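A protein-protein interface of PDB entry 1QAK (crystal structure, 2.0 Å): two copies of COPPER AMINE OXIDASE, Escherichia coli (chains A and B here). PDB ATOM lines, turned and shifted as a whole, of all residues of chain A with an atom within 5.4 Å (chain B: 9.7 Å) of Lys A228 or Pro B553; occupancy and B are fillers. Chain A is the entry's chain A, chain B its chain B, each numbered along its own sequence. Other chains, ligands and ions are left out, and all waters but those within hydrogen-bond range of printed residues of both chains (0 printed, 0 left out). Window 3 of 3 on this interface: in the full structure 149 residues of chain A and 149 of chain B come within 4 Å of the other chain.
CB of Pro B553 touches CD1 of Phe A225, at 3.7 Å.
CG of Pro B553 touches O of Lys A228 (3.8 Å).
Tyr A372 touches Pro B553.
NH1 of Arg B554 is in hydrogen-bond range of O of Tyr A372.
The guanidinium group of Arg B554 is in salt-bridge range of the side-chain carboxylate of Glu A620, at 2.9 Å.
N of Thr B555 is in hydrogen-bond range of OE1 of Glu A620 (2.9 Å).
OE2 of Glu A620 sits at hydrogen-bond distance from N of Ser B556.
No position is printed for both chains.
Of the 7 pairs that touch across the chains among the printed residues, none has its exchanged pair printed and touching as well.
Lys A228 touches just one residue of chain B: Pro B553.
Of the printed residues of chain B, Tyr A372 touches Pro B553 (3.4 Å) and Arg B554 (3.0 Å).
Printed residues of chain B within 4 Å of Glu A620: Arg B554 (2.9 Å), Thr B555 (2.9 Å) and Ser B556 (2.7 Å).
Thr B549 touches none of the printed residues of chain A.
Pro B553 touches just these residues of chain A: Phe A225 (3.7 Å), Lys A228 (3.8 Å) and Tyr A372 (3.4 Å).
Of the printed residues of chain A, Ser B556 touches Glu A620 (2.7 Å).
Of the 10 printed residues of chain B, 4 touch a printed residue of chain A.
Printed residues of chain B that touch a printed residue of chain A: Pro B553, Arg B554, Thr B555 and Ser B556.
Hydrophobic or aromatic side chains of chain B that line the printed part of chain A: Pro B553.
Of the 8 printed residues of chain A, 4 touch a printed residue of chain B.
Hydrophobic or aromatic side chains of chain A within 4 Å of the printed part of chain B: Phe A225 and Tyr A372.
Among the printed residues, 7 pairs touch across the chains.
Among the printed residues, Asp or Glu carboxylates within 4 Å of a Lys or Arg side-chain nitrogen of the other chain: Glu A620 with Arg B554 (2.9 Å).
OD1 of Asn B548 sits close to O of Arg B554.
O of Thr B555 lies within hydrogen-bond range of N of Asn B548 (2.9 Å).
The guanidinium group (NE) of Arg B554 is in hydrogen-bond range of the backbone carbonyl oxygen (O) of Ser B556 (3.3 Å).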
ATOM      1  N   PHE A 225     -15.022  27.186  -2.571  1.00  0.00           N
ATOM      2  CA  PHE A 225     -13.722  27.712  -2.967  1.00  0.00           C
ATOM      3  C   PHE A 225     -13.859  28.818  -4.015  1.00  0.00           C
ATOM      4  O   PHE A 225     -12.970  28.954  -4.860  1.00  0.00           O
ATOM      5  CB  PHE A 225     -12.936  26.535  -3.579  1.00  0.00           C
ATOM      6  CG  PHE A 225     -12.588  25.534  -2.516  1.00  0.00           C
ATOM      7  CD1 PHE A 225     -11.431  25.694  -1.771  1.00  0.00           C
ATOM      8  CD2 PHE A 225     -13.425  24.459  -2.245  1.00  0.00           C
ATOM      9  CE1 PHE A 225     -11.089  24.808  -0.774  1.00  0.00           C
ATOM     10  CE2 PHE A 225     -13.091  23.558  -1.257  1.00  0.00           C
ATOM     11  CZ  PHE A 225     -11.933  23.731  -0.512  1.00  0.00           C
ATOM     12  N   ASP A 226     -14.945  29.570  -3.949  1.00  0.00           N
ATOM     13  CA  ASP A 226     -15.239  30.674  -4.855  1.00  0.00           C
ATOM     14  C   ASP A 226     -15.021  30.245  -6.296  1.00  0.00           C
ATOM     15  O   ASP A 226     -14.369  30.943  -7.068  1.00  0.00           O
ATOM     16  CB  ASP A 226     -14.302  31.832  -4.511  1.00  0.00           C
ATOM     17  CG  ASP A 226     -14.711  33.215  -4.976  1.00  0.00           C
ATOM     18  OD1 ASP A 226     -15.894  33.539  -5.207  1.00  0.00           O
ATOM     19  OD2 ASP A 226     -13.727  33.986  -5.081  1.00  0.00           O
ATOM     20  N   GLY A 227     -15.540  29.085  -6.666  1.00  0.00           N
ATOM     21  CA  GLY A 227     -15.417  28.588  -8.025  1.00  0.00           C
ATOM     22  C   GLY A 227     -14.107  27.931  -8.382  1.00  0.00           C
ATOM     23  O   GLY A 227     -14.099  27.271  -9.421  1.00  0.00           O
ATOM     24  N   LYS A 228     -13.077  28.057  -7.572  1.00  0.00           N
ATOM     25  CA  LYS A 228     -11.796  27.438  -7.909  1.00  0.00           C
ATOM     26  C   LYS A 228     -11.842  25.928  -7.982  1.00  0.00           C
ATOM     27  O   LYS A 228     -10.935  25.272  -8.538  1.00  0.00           O
ATOM     28  CB  LYS A 228     -10.711  27.905  -6.938  1.00  0.00           C
ATOM     29  CG  LYS A 228     -10.718  29.431  -6.896  1.00  0.00           C
ATOM     30  CD  LYS A 228     -10.001  29.977  -8.125  1.00  0.00           C
ATOM     31  CE  LYS A 228      -9.211  31.228  -7.766  1.00  0.00           C
ATOM     32  NZ  LYS A 228      -7.754  31.001  -7.520  1.00  0.00           N
ATOM     33  N   ASP A 229     -12.919  25.384  -7.394  1.00  0.00           N
ATOM     34  CA  ASP A 229     -12.964  23.912  -7.471  1.00  0.00           C
ATOM     35  C   ASP A 229     -13.756  23.489  -8.716  1.00  0.00           C
ATOM     36  O   ASP A 229     -13.947  22.281  -8.934  1.00  0.00           O
ATOM     37  CB  ASP A 229     -13.607  23.274  -6.239  1.00  0.00           C
ATOM     38  CG  ASP A 229     -14.941  23.874  -5.899  1.00  0.00           C
ATOM     39  OD1 ASP A 229     -15.405  24.811  -6.578  1.00  0.00           O
ATOM     40  OD2 ASP A 229     -15.538  23.387  -4.907  1.00  0.00           O
ATOM     41  N   GLY A 230     -14.175  24.533  -9.440  1.00  0.00           N
ATOM     42  CA  GLY A 230     -14.947  24.312 -10.664  1.00  0.00           C
ATOM     43  C   GLY A 230     -16.384  23.911 -10.369  1.00  0.00           C
ATOM     44  O   GLY A 230     -17.098  23.446 -11.264  1.00  0.00           O
ATOM     45  N   TYR A 372      -7.904  18.138  -0.390  1.00  0.00           N
ATOM     46  CA  TYR A 372      -8.015  19.574  -0.193  1.00  0.00           C
ATOM     47  C   TYR A 372      -9.343  20.129   0.273  1.00  0.00           C
ATOM     48  O   TYR A 372      -9.278  21.154   0.960  1.00  0.00           O
ATOM     49  CB  TYR A 372      -7.559  20.292  -1.469  1.00  0.00           C
ATOM     50  CG  TYR A 372      -8.611  20.518  -2.534  1.00  0.00           C
ATOM     51  CD1 TYR A 372      -9.563  21.521  -2.414  1.00  0.00           C
ATOM     52  CD2 TYR A 372      -8.612  19.692  -3.658  1.00  0.00           C
ATOM     53  CE1 TYR A 372     -10.502  21.690  -3.425  1.00  0.00           C
ATOM     54  CE2 TYR A 372      -9.548  19.869  -4.665  1.00  0.00           C
ATOM     55  CZ  TYR A 372     -10.483  20.872  -4.544  1.00  0.00           C
ATOM     56  OH  TYR A 372     -11.435  21.064  -5.536  1.00  0.00           O
ATOM     57  N   GLU A 620      -7.514  30.885   3.664  1.00  0.00           N
ATOM     58  CA  GLU A 620      -8.180  29.660   3.247  1.00  0.00           C
ATOM     59  C   GLU A 620      -9.692  29.832   3.334  1.00  0.00           C
ATOM     60  O   GLU A 620     -10.190  30.515   4.228  1.00  0.00           O
ATOM     61  CB  GLU A 620      -7.757  28.433   4.063  1.00  0.00           C
ATOM     62  CG  GLU A 620      -6.303  28.063   3.831  1.00  0.00           C
ATOM     63  CD  GLU A 620      -5.993  27.162   2.669  1.00  0.00           C
ATOM     64  OE1 GLU A 620      -6.712  27.394   1.671  1.00  0.00           O
ATOM     65  OE2 GLU A 620      -5.092  26.298   2.784  1.00  0.00           O
ATOM     66  N   ASN B 548       0.926  26.138   0.203  1.00  0.00           N
ATOM     67  CA  ASN B 548       0.632  24.994  -0.631  1.00  0.00           C
ATOM     68  C   ASN B 548       1.433  25.184  -1.929  1.00  0.00           C
ATOM     69  O   ASN B 548       1.213  26.209  -2.546  1.00  0.00           O
ATOM     70  CB  ASN B 548      -0.867  24.945  -0.974  1.00  0.00           C
ATOM     71  CG  ASN B 548      -1.188  23.882  -2.016  1.00  0.00           C
ATOM     72  OD1 ASN B 548      -2.183  23.994  -2.729  1.00  0.00           O
ATOM     73  ND2 ASN B 548      -0.340  22.884  -2.082  1.00  0.00           N
ATOM     74  N   THR B 549       2.286  24.243  -2.284  1.00  0.00           N
ATOM     75  CA  THR B 549       3.044  24.386  -3.528  1.00  0.00           C
ATOM     76  C   THR B 549       2.685  23.234  -4.466  1.00  0.00           C
ATOM     77  O   THR B 549       3.289  23.008  -5.517  1.00  0.00           O
ATOM     78  CB  THR B 549       4.565  24.360  -3.311  1.00  0.00           C
ATOM     79  OG1 THR B 549       4.867  23.062  -2.801  1.00  0.00           O
ATOM     80  CG2 THR B 549       5.048  25.447  -2.370  1.00  0.00           C
ATOM     81  N   ALA B 550       1.662  22.457  -4.111  1.00  0.00           N
ATOM     82  CA  ALA B 550       1.241  21.345  -4.934  1.00  0.00           C
ATOM     83  C   ALA B 550       0.117  21.653  -5.916  1.00  0.00           C
ATOM     84  O   ALA B 550      -0.277  20.716  -6.620  1.00  0.00           O
ATOM     85  CB  ALA B 550       0.792  20.136  -4.123  1.00  0.00           C
ATOM     86  N   GLY B 551      -0.379  22.859  -5.989  1.00  0.00           N
ATOM     87  CA  GLY B 551      -1.458  23.203  -6.910  1.00  0.00           C
ATOM     88  C   GLY B 551      -2.818  22.914  -6.272  1.00  0.00           C
ATOM     89  O   GLY B 551      -2.954  22.362  -5.177  1.00  0.00           O
ATOM     90  N   GLY B 552      -3.878  23.283  -6.965  1.00  0.00           N
ATOM     91  CA  GLY B 552      -5.260  23.079  -6.522  1.00  0.00           C
ATOM     92  C   GLY B 552      -5.664  24.325  -5.754  1.00  0.00           C
ATOM     93  O   GLY B 552      -4.869  25.233  -5.574  1.00  0.00           O
ATOM     94  N   PRO B 553      -6.903  24.389  -5.296  1.00  0.00           N
ATOM     95  CA  PRO B 553      -7.409  25.542  -4.574  1.00  0.00           C
ATOM     96  C   PRO B 553      -6.804  25.902  -3.225  1.00  0.00           C
ATOM     97  O   PRO B 553      -6.874  27.083  -2.839  1.00  0.00           O
ATOM     98  CB  PRO B 553      -8.924  25.259  -4.413  1.00  0.00           C
ATOM     99  CG  PRO B 553      -9.159  24.105  -5.342  1.00  0.00           C
ATOM    100  CD  PRO B 553      -7.886  23.322  -5.512  1.00  0.00           C
ATOM    101  N   ARG B 554      -6.228  24.957  -2.477  1.00  0.00           N
ATOM    102  CA  ARG B 554      -5.689  25.342  -1.169  1.00  0.00           C
ATOM    103  C   ARG B 554      -4.505  26.311  -1.147  1.00  0.00           C
ATOM    104  O   ARG B 554      -3.632  26.180  -1.996  1.00  0.00           O
ATOM    105  CB  ARG B 554      -5.272  24.149  -0.291  1.00  0.00           C
ATOM    106  CG  ARG B 554      -6.401  23.250   0.232  1.00  0.00           C
ATOM    107  CD  ARG B 554      -7.041  23.913   1.467  1.00  0.00           C
ATOM    108  NE  ARG B 554      -6.216  23.625   2.652  1.00  0.00           N
ATOM    109  CZ  ARG B 554      -6.182  22.460   3.280  1.00  0.00           C
ATOM    110  NH1 ARG B 554      -6.928  21.431   2.872  1.00  0.00           N
ATOM    111  NH2 ARG B 554      -5.393  22.305   4.334  1.00  0.00           N
ATOM    112  N   THR B 555      -4.490  27.223  -0.169  1.00  0.00           N
ATOM    113  CA  THR B 555      -3.334  28.142  -0.134  1.00  0.00           C
ATOM    114  C   THR B 555      -2.284  27.655   0.855  1.00  0.00           C
ATOM    115  O   THR B 555      -1.133  28.075   0.841  1.00  0.00           O
ATOM    116  CB  THR B 555      -3.739  29.565   0.276  1.00  0.00           C
ATOM    117  OG1 THR B 555      -4.153  29.536   1.644  1.00  0.00           O
ATOM    118  CG2 THR B 555      -4.891  30.082  -0.575  1.00  0.00           C
ATOM    119  N   SER B 556      -2.614  26.729   1.752  1.00  0.00           N
ATOM    120  CA  SER B 556      -1.727  26.189   2.769  1.00  0.00           C
ATOM    121  C   SER B 556      -1.947  24.712   3.046  1.00  0.00           C
ATOM    122  O   SER B 556      -2.896  24.048   2.650  1.00  0.00           O
ATOM    123  CB  SER B 556      -1.923  26.934   4.091  1.00  0.00           C
ATOM    124  OG  SER B 556      -3.223  26.864   4.694  1.00  0.00           O
ATOM    125  N   THR B 557      -0.993  24.148   3.761  1.00  0.00           N
ATOM    126  CA  THR B 557      -0.944  22.768   4.150  1.00  0.00           C
ATOM    127  C   THR B 557      -0.461  22.608   5.580  1.00  0.00           C
ATOM    128  O   THR B 557       0.091  23.598   6.100  1.00  0.00           O
ATOM    129  CB  THR B 557       0.021  21.983   3.223  1.00  0.00           C
ATOM    130  OG1 THR B 557       1.373  22.378   3.512  1.00  0.00           O
ATOM    131  CG2 THR B 557      -0.343  22.185   1.757  1.00  0.00           C
